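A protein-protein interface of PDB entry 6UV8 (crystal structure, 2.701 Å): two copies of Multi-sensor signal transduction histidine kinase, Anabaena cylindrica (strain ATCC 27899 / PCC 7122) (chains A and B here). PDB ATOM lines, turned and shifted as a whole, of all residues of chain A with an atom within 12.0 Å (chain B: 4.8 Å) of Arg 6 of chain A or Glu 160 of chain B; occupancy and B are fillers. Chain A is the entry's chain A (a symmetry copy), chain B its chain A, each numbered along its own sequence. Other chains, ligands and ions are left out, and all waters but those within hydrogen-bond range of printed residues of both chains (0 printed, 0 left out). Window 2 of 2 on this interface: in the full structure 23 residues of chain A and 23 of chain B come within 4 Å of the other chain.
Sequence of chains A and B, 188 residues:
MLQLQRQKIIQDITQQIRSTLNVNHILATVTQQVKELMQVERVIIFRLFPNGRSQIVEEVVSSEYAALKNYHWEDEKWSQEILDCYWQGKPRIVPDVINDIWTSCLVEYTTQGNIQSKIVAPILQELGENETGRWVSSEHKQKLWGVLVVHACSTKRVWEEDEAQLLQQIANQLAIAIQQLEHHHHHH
No position is printed for both chains.
The guanidinium group (NH1) of Arg 6 of chain A lies within salt-bridge range of the side-chain carboxylate (OE1) of Glu 160 of chain B (2.5 Å). The side-chain carboxylate (OD2) of Asp 162 of chain B lies within hydrogen-bond range of the side-chain amide nitrogen (NE2) of Gln 3 of chain A. OE2 of Glu 163 of chain B lies within salt-bridge range of NH1 of Arg 6 of chain A (3.9 Å).
The backbone NH (N) of Glu 160 of chain B is in hydrogen-bond range of the side-chain carboxylate (OE1) of Glu 163 of chain B, at 3.0 Å. The side-chain carboxylate of Asp 162 of chain B sits close to the side-chain carboxylate of Glu 161 of chain B (2.7 Å).
Among the printed residues, merely in contact across the chains: Arg 6 of chain A with Leu 37 of chain B (3.9 Å) and Ile 9 of chain A with Leu 37 of chain B (3.5 Å).
Of the printed residues of chain B, Arg 6 of chain A touches Leu 37 (3.9 Å), Glu 160 (2.5 Å) and Glu 163 (3.9 Å). Of chain A, only Arg 6 (2.5 Å) comes within 4 Å of Glu 160 of chain B. No residue of chain A comes within 4 Å of Val 158 of chain B. Trp 159 of chain B touches none of the printed residues of chain A. No residue of chain A comes within 4 Å of Glu 161 of chain B. Glu 163 of chain B touches just one residue of chain A: Arg 6. Printed residues of chain B within 4 Å of Ile 9 of chain A: Leu 37. Of the printed residues of chain B, Gln 3 of chain A touches Asp 162. Of the printed residues of chain A, Leu 37 of chain B touches Arg 6 (3.9 Å) and Ile 9 (3.5 Å). Thr 14 of chain A touches none of the printed residues of chain B. The nearest printed residue of chain A that does not touch Leu 37 of chain B is Ile 13 of chain A (4.8 Å).
Of the 16 printed residues of chain A, 3 touch a printed residue of chain B. Hydrophobic or aromatic side chains of chain A that line the printed part of chain B: Ile 9. Of the 9 printed residues of chain B, 4 touch a printed residue of chain A. Hydrophobic or aromatic side chains of chain B that line the printed part of chain A: Leu 37. Among the printed residues, 5 pairs touch across the chains.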
ATOM      1  N   MET A   1     -15.595   5.371   4.308  1.00  0.00           N
ATOM      2  CA  MET A   1     -14.598   5.859   3.370  1.00  0.00           C
ATOM      3  C   MET A   1     -14.516   4.879   2.209  1.00  0.00           C
ATOM      4  O   MET A   1     -15.482   4.179   1.907  1.00  0.00           O
ATOM      5  CB  MET A   1     -13.234   6.022   4.060  1.00  0.00           C
ATOM      6  CG  MET A   1     -12.215   6.908   3.337  1.00  0.00           C
ATOM      7  SD  MET A   1     -12.660   8.645   3.240  1.00  0.00           S
ATOM      8  CE  MET A   1     -12.272   9.175   4.901  1.00  0.00           C
ATOM      9  N   LEU A   2     -13.355   4.840   1.564  1.00  0.00           N
ATOM     10  CA  LEU A   2     -13.073   3.896   0.497  1.00  0.00           C
ATOM     11  C   LEU A   2     -12.607   2.542   1.022  1.00  0.00           C
ATOM     12  O   LEU A   2     -12.213   1.689   0.218  1.00  0.00           O
ATOM     13  CB  LEU A   2     -12.026   4.484  -0.455  1.00  0.00           C
ATOM     14  CG  LEU A   2     -12.079   4.037  -1.916  1.00  0.00           C
ATOM     15  CD1 LEU A   2     -13.499   4.106  -2.455  1.00  0.00           C
ATOM     16  CD2 LEU A   2     -11.155   4.902  -2.753  1.00  0.00           C
ATOM     17  N   GLN A   3     -12.651   2.322   2.341  1.00  0.00           N
ATOM     18  CA  GLN A   3     -12.550   0.979   2.908  1.00  0.00           C
ATOM     19  C   GLN A   3     -13.623   0.103   2.272  1.00  0.00           C
ATOM     20  O   GLN A   3     -13.520  -1.129   2.240  1.00  0.00           O
ATOM     21  CB  GLN A   3     -12.703   1.034   4.430  1.00  0.00           C
ATOM     22  CG  GLN A   3     -12.665  -0.318   5.142  1.00  0.00           C
ATOM     23  CD  GLN A   3     -12.446  -0.184   6.640  1.00  0.00           C
ATOM     24  OE1 GLN A   3     -12.039   0.874   7.130  1.00  0.00           O
ATOM     25  NE2 GLN A   3     -12.716  -1.258   7.376  1.00  0.00           N
ATOM     26  N   LEU A   4     -14.670   0.767   1.784  1.00  0.00           N
ATOM     27  CA  LEU A   4     -15.632   0.164   0.872  1.00  0.00           C
ATOM     28  C   LEU A   4     -14.948  -0.607  -0.257  1.00  0.00           C
ATOM     29  O   LEU A   4     -15.331  -1.741  -0.561  1.00  0.00           O
ATOM     30  CB  LEU A   4     -16.524   1.280   0.324  1.00  0.00           C
ATOM     31  CG  LEU A   4     -17.481   1.112  -0.851  1.00  0.00           C
ATOM     32  CD1 LEU A   4     -18.673   0.272  -0.445  1.00  0.00           C
ATOM     33  CD2 LEU A   4     -17.918   2.491  -1.324  1.00  0.00           C
ATOM     34  N   GLN A   5     -13.925  -0.015  -0.885  1.00  0.00           N
ATOM     35  CA  GLN A   5     -13.298  -0.643  -2.049  1.00  0.00           C
ATOM     36  C   GLN A   5     -12.427  -1.847  -1.690  1.00  0.00           C
ATOM     37  O   GLN A   5     -12.247  -2.737  -2.533  1.00  0.00           O
ATOM     38  CB  GLN A   5     -12.471   0.390  -2.829  1.00  0.00           C
ATOM     39  CG  GLN A   5     -11.904  -0.116  -4.164  1.00  0.00           C
ATOM     40  CD  GLN A   5     -12.980  -0.578  -5.141  1.00  0.00           C
ATOM     41  OE1 GLN A   5     -12.917  -1.687  -5.684  1.00  0.00           O
ATOM     42  NE2 GLN A   5     -13.968   0.278  -5.377  1.00  0.00           N
ATOM     43  N   ARG A   6     -11.889  -1.901  -0.467  1.00  0.00           N
ATOM     44  CA  ARG A   6     -11.120  -3.070  -0.050  1.00  0.00           C
ATOM     45  C   ARG A   6     -11.936  -4.344  -0.219  1.00  0.00           C
ATOM     46  O   ARG A   6     -11.458  -5.339  -0.776  1.00  0.00           O
ATOM     47  CB  ARG A   6     -10.661  -2.916   1.403  1.00  0.00           C
ATOM     48  CG  ARG A   6      -9.649  -1.812   1.644  1.00  0.00           C
ATOM     49  CD  ARG A   6      -8.830  -2.102   2.887  1.00  0.00           C
ATOM     50  NE  ARG A   6      -7.915  -1.014   3.209  1.00  0.00           N
ATOM     51  CZ  ARG A   6      -8.113  -0.137   4.187  1.00  0.00           C
ATOM     52  NH1 ARG A   6      -7.225   0.824   4.408  1.00  0.00           N
ATOM     53  NH2 ARG A   6      -9.192  -0.227   4.949  1.00  0.00           N
ATOM     54  N   GLN A   7     -13.188  -4.320   0.225  1.00  0.00           N
ATOM     55  CA  GLN A   7     -14.011  -5.516   0.168  1.00  0.00           C
ATOM     56  C   GLN A   7     -14.552  -5.808  -1.224  1.00  0.00           C
ATOM     57  O   GLN A   7     -14.892  -6.961  -1.508  1.00  0.00           O
ATOM     58  CB  GLN A   7     -15.165  -5.405   1.158  1.00  0.00           C
ATOM     59  CG  GLN A   7     -14.722  -5.084   2.567  1.00  0.00           C
ATOM     60  CD  GLN A   7     -15.763  -5.471   3.589  1.00  0.00           C
ATOM     61  OE1 GLN A   7     -16.156  -4.661   4.435  1.00  0.00           O
ATOM     62  NE2 GLN A   7     -16.221  -6.721   3.520  1.00  0.00           N
ATOM     63  N   LYS A   8     -14.640  -4.804  -2.101  1.00  0.00           N
ATOM     64  CA  LYS A   8     -15.106  -5.063  -3.458  1.00  0.00           C
ATOM     65  C   LYS A   8     -14.169  -5.973  -4.224  1.00  0.00           C
ATOM     66  O   LYS A   8     -14.534  -6.438  -5.306  1.00  0.00           O
ATOM     67  CB  LYS A   8     -15.286  -3.762  -4.241  1.00  0.00           C
ATOM     68  CG  LYS A   8     -16.704  -3.211  -4.211  1.00  0.00           C
ATOM     69  CD  LYS A   8     -16.796  -1.888  -4.961  1.00  0.00           C
ATOM     70  CE  LYS A   8     -17.896  -0.997  -4.393  1.00  0.00           C
ATOM     71  NZ  LYS A   8     -17.752   0.425  -4.832  1.00  0.00           N
ATOM     72  N   ILE A   9     -12.979  -6.231  -3.698  1.00  0.00           N
ATOM     73  CA  ILE A   9     -12.112  -7.222  -4.309  1.00  0.00           C
ATOM     74  C   ILE A   9     -12.103  -8.476  -3.447  1.00  0.00           C
ATOM     75  O   ILE A   9     -11.975  -9.587  -3.968  1.00  0.00           O
ATOM     76  CB  ILE A   9     -10.694  -6.672  -4.527  1.00  0.00           C
ATOM     77  CG1 ILE A   9      -9.890  -7.646  -5.383  1.00  0.00           C
ATOM     78  CG2 ILE A   9     -10.011  -6.444  -3.218  1.00  0.00           C
ATOM     79  CD1 ILE A   9     -10.569  -7.977  -6.689  1.00  0.00           C
ATOM     80  N   ILE A  10     -12.256  -8.321  -2.128  1.00  0.00           N
ATOM     81  CA  ILE A  10     -12.270  -9.503  -1.269  1.00  0.00           C
ATOM     82  C   ILE A  10     -13.439 -10.396  -1.642  1.00  0.00           C
ATOM     83  O   ILE A  10     -13.325 -11.628  -1.650  1.00  0.00           O
ATOM     84  CB  ILE A  10     -12.298  -9.117   0.223  1.00  0.00           C
ATOM     85  CG1 ILE A  10     -11.667 -10.239   1.054  1.00  0.00           C
ATOM     86  CG2 ILE A  10     -13.714  -8.887   0.725  1.00  0.00           C
ATOM     87  CD1 ILE A  10     -12.613 -10.936   2.026  1.00  0.00           C
ATOM     88  N   GLN A  11     -14.571  -9.790  -1.998  1.00  0.00           N
ATOM     89  CA  GLN A  11     -15.703 -10.580  -2.446  1.00  0.00           C
ATOM     90  C   GLN A  11     -15.417 -11.198  -3.804  1.00  0.00           C
ATOM     91  O   GLN A  11     -15.862 -12.317  -4.082  1.00  0.00           O
ATOM     92  CB  GLN A  11     -16.961  -9.710  -2.468  1.00  0.00           C
ATOM     93  CG  GLN A  11     -18.205 -10.400  -2.984  1.00  0.00           C
ATOM     94  CD  GLN A  11     -18.600  -9.889  -4.349  1.00  0.00           C
ATOM     95  OE1 GLN A  11     -18.483  -8.692  -4.628  1.00  0.00           O
ATOM     96  NE2 GLN A  11     -19.055 -10.791  -5.217  1.00  0.00           N
ATOM     97  N   ASP A  12     -14.654 -10.501  -4.649  1.00  0.00           N
ATOM     98  CA  ASP A  12     -14.159 -11.119  -5.871  1.00  0.00           C
ATOM     99  C   ASP A  12     -13.264 -12.303  -5.547  1.00  0.00           C
ATOM    100  O   ASP A  12     -13.522 -13.425  -5.988  1.00  0.00           O
ATOM    101  CB  ASP A  12     -13.409 -10.094  -6.720  1.00  0.00           C
ATOM    102  CG  ASP A  12     -14.341  -9.199  -7.500  1.00  0.00           C
ATOM    103  OD1 ASP A  12     -15.270  -9.741  -8.137  1.00  0.00           O
ATOM    104  OD2 ASP A  12     -14.148  -7.963  -7.473  1.00  0.00           O
ATOM    105  N   ILE A  13     -12.225 -12.073  -4.741  1.00  0.00           N
ATOM    106  CA  ILE A  13     -11.254 -13.125  -4.441  1.00  0.00           C
ATOM    107  C   ILE A  13     -11.952 -14.355  -3.887  1.00  0.00           C
ATOM    108  O   ILE A  13     -11.738 -15.478  -4.354  1.00  0.00           O
ATOM    109  CB  ILE A  13     -10.182 -12.607  -3.468  1.00  0.00           C
ATOM    110  CG1 ILE A  13      -9.298 -11.579  -4.161  1.00  0.00           C
ATOM    111  CG2 ILE A  13      -9.361 -13.757  -2.937  1.00  0.00           C
ATOM    112  CD1 ILE A  13      -8.534 -10.698  -3.214  1.00  0.00           C
ATOM    113  N   THR A  14     -12.797 -14.166  -2.877  1.00  0.00           N
ATOM    114  CA  THR A  14     -13.568 -15.293  -2.379  1.00  0.00           C
ATOM    115  C   THR A  14     -14.392 -15.910  -3.491  1.00  0.00           C
ATOM    116  O   THR A  14     -14.444 -17.135  -3.623  1.00  0.00           O
ATOM    117  CB  THR A  14     -14.478 -14.859  -1.240  1.00  0.00           C
ATOM    118  OG1 THR A  14     -13.766 -13.968  -0.380  1.00  0.00           O
ATOM    119  CG2 THR A  14     -14.926 -16.075  -0.446  1.00  0.00           C
ATOM    120  N   GLN A  15     -15.026 -15.070  -4.313  1.00  0.00           N
ATOM    121  CA  GLN A  15     -15.892 -15.571  -5.376  1.00  0.00           C
ATOM    122  C   GLN A  15     -15.148 -16.531  -6.293  1.00  0.00           C
ATOM    123  O   GLN A  15     -15.705 -17.544  -6.722  1.00  0.00           O
ATOM    124  CB  GLN A  15     -16.466 -14.403  -6.183  1.00  0.00           C
ATOM    125  CG  GLN A  15     -17.621 -14.768  -7.105  1.00  0.00           C
ATOM    126  CD  GLN A  15     -18.950 -14.878  -6.371  1.00  0.00           C
ATOM    127  OE1 GLN A  15     -19.368 -13.949  -5.673  1.00  0.00           O
ATOM    128  NE2 GLN A  15     -19.621 -16.017  -6.528  1.00  0.00           N
ATOM    129  N   GLN A  16     -13.883 -16.239  -6.597  1.00  0.00           N
ATOM    130  CA  GLN A  16     -13.127 -17.125  -7.475  1.00  0.00           C
ATOM    131  C   GLN A  16     -12.721 -18.404  -6.761  1.00  0.00           C
ATOM    132  O   GLN A  16     -12.870 -19.497  -7.318  1.00  0.00           O
ATOM    133  CB  GLN A  16     -11.897 -16.406  -8.029  1.00  0.00           C
ATOM    134  CG  GLN A  16     -12.244 -15.298  -9.014  1.00  0.00           C
ATOM    135  CD  GLN A  16     -12.116 -13.914  -8.405  1.00  0.00           C
ATOM    136  OE1 GLN A  16     -11.237 -13.675  -7.581  1.00  0.00           O
ATOM    137  NE2 GLN A  16     -13.007 -12.998  -8.794  1.00  0.00           N
ATOM    138  N   LEU B  37      -4.092  -4.813  -4.452  1.00  0.00           N
ATOM    139  CA  LEU B  37      -5.143  -4.284  -3.593  1.00  0.00           C
ATOM    140  C   LEU B  37      -4.583  -3.478  -2.426  1.00  0.00           C
ATOM    141  O   LEU B  37      -5.041  -2.362  -2.167  1.00  0.00           O
ATOM    142  CB  LEU B  37      -6.014  -5.432  -3.075  1.00  0.00           C
ATOM    143  CG  LEU B  37      -6.640  -5.285  -1.689  1.00  0.00           C
ATOM    144  CD1 LEU B  37      -7.761  -4.258  -1.685  1.00  0.00           C
ATOM    145  CD2 LEU B  37      -7.133  -6.627  -1.191  1.00  0.00           C
ATOM    146  N   ILE B  93       0.768  -7.860  13.132  1.00  0.00           N
ATOM    147  CA  ILE B  93       1.195  -6.600  12.539  1.00  0.00           C
ATOM    148  C   ILE B  93       2.574  -6.257  13.072  1.00  0.00           C
ATOM    149  O   ILE B  93       2.775  -6.127  14.285  1.00  0.00           O
ATOM    150  CB  ILE B  93       0.202  -5.466  12.809  1.00  0.00           C
ATOM    151  CG1 ILE B  93      -1.169  -5.829  12.242  1.00  0.00           C
ATOM    152  CG2 ILE B  93       0.722  -4.205  12.159  1.00  0.00           C
ATOM    153  CD1 ILE B  93      -2.054  -4.647  12.000  1.00  0.00           C
ATOM    154  N   VAL B 158       2.240   2.186   8.382  1.00  0.00           N
ATOM    155  CA  VAL B 158       1.361   1.901   9.504  1.00  0.00           C
ATOM    156  C   VAL B 158       0.143   1.174   8.972  1.00  0.00           C
ATOM    157  O   VAL B 158      -0.377   1.496   7.897  1.00  0.00           O
ATOM    158  CB  VAL B 158       0.966   3.191  10.238  1.00  0.00           C
ATOM    159  CG1 VAL B 158       2.140   3.695  11.057  1.00  0.00           C
ATOM    160  CG2 VAL B 158       0.494   4.249   9.243  1.00  0.00           C
ATOM    161  N   TRP B 159      -0.308   0.177   9.716  1.00  0.00           N
ATOM    162  CA  TRP B 159      -1.367  -0.707   9.259  1.00  0.00           C
ATOM    163  C   TRP B 159      -2.609  -0.496  10.109  1.00  0.00           C
ATOM    164  O   TRP B 159      -2.519  -0.473  11.340  1.00  0.00           O
ATOM    165  CB  TRP B 159      -0.925  -2.173   9.336  1.00  0.00           C
ATOM    166  CG  TRP B 159       0.374  -2.495   8.648  1.00  0.00           C
ATOM    167  CD1 TRP B 159       1.608  -2.619   9.232  1.00  0.00           C
ATOM    168  CD2 TRP B 159       0.563  -2.751   7.254  1.00  0.00           C
ATOM    169  NE1 TRP B 159       2.549  -2.931   8.280  1.00  0.00           N
ATOM    170  CE2 TRP B 159       1.933  -3.016   7.060  1.00  0.00           C
ATOM    171  CE3 TRP B 159      -0.292  -2.771   6.149  1.00  0.00           C
ATOM    172  CZ2 TRP B 159       2.461  -3.301   5.811  1.00  0.00           C
ATOM    173  CZ3 TRP B 159       0.231  -3.066   4.919  1.00  0.00           C
ATOM    174  CH2 TRP B 159       1.594  -3.322   4.755  1.00  0.00           C
ATOM    175  N   GLU B 160      -3.759  -0.341   9.460  1.00  0.00           N
ATOM    176  CA  GLU B 160      -5.016  -0.329  10.191  1.00  0.00           C
ATOM    177  C   GLU B 160      -5.424  -1.765  10.508  1.00  0.00           C
ATOM    178  O   GLU B 160      -5.092  -2.697   9.765  1.00  0.00           O
ATOM    179  CB  GLU B 160      -6.117   0.364   9.383  1.00  0.00           C
ATOM    180  CG  GLU B 160      -5.676   1.608   8.630  1.00  0.00           C
ATOM    181  CD  GLU B 160      -6.564   1.899   7.430  1.00  0.00           C
ATOM    182  OE1 GLU B 160      -6.035   2.041   6.301  1.00  0.00           O
ATOM    183  OE2 GLU B 160      -7.798   1.964   7.617  1.00  0.00           O
ATOM    184  N   GLU B 161      -6.141  -1.941  11.631  1.00  0.00           N
ATOM    185  CA  GLU B 161      -6.584  -3.282  12.009  1.00  0.00           C
ATOM    186  C   GLU B 161      -7.332  -3.937  10.866  1.00  0.00           C
ATOM    187  O   GLU B 161      -7.183  -5.139  10.626  1.00  0.00           O
ATOM    188  CB  GLU B 161      -7.466  -3.257  13.268  1.00  0.00           C
ATOM    189  CG  GLU B 161      -8.928  -2.756  13.074  1.00  0.00           C
ATOM    190  CD  GLU B 161      -9.983  -3.840  12.712  1.00  0.00           C
ATOM    191  OE1 GLU B 161      -9.830  -5.012  13.097  1.00  0.00           O
ATOM    192  OE2 GLU B 161     -10.986  -3.502  12.053  1.00  0.00           O
ATOM    193  N   ASP B 162      -8.118  -3.149  10.128  1.00  0.00           N
ATOM    194  CA  ASP B 162      -8.903  -3.710   9.039  1.00  0.00           C
ATOM    195  C   ASP B 162      -8.000  -4.233   7.937  1.00  0.00           C
ATOM    196  O   ASP B 162      -8.374  -5.171   7.228  1.00  0.00           O
ATOM    197  CB  ASP B 162      -9.897  -2.668   8.513  1.00  0.00           C
ATOM    198  CG  ASP B 162     -10.979  -2.328   9.540  1.00  0.00           C
ATOM    199  OD1 ASP B 162     -10.741  -1.429  10.371  1.00  0.00           O
ATOM    200  OD2 ASP B 162     -12.048  -2.979   9.539  1.00  0.00           O
ATOM    201  N   GLU B 163      -6.799  -3.664   7.802  1.00  0.00           N
ATOM    202  CA  GLU B 163      -5.844  -4.170   6.822  1.00  0.00           C
ATOM    203  C   GLU B 163      -5.409  -5.580   7.186  1.00  0.00           C
ATOM    204  O   GLU B 163      -5.522  -6.505   6.374  1.00  0.00           O
ATOM    205  CB  GLU B 163      -4.641  -3.226   6.715  1.00  0.00           C
ATOM    206  CG  GLU B 163      -4.707  -2.274   5.520  1.00  0.00           C
ATOM    207  CD  GLU B 163      -3.688  -1.145   5.585  1.00  0.00           C
ATOM    208  OE1 GLU B 163      -3.068  -0.959   6.651  1.00  0.00           O
ATOM    209  OE2 GLU B 163      -3.516  -0.433   4.569  1.00  0.00           O
ATOM    210  N   ALA B 164      -4.947  -5.772   8.426  1.00  0.00           N
ATOM    211  CA  ALA B 164      -4.632  -7.114   8.916  1.00  0.00           C
ATOM    212  C   ALA B 164      -5.859  -8.011   8.875  1.00  0.00           C
ATOM    213  O   ALA B 164      -5.807  -9.131   8.354  1.00  0.00           O
ATOM    214  CB  ALA B 164      -4.093  -7.039  10.346  1.00  0.00           C
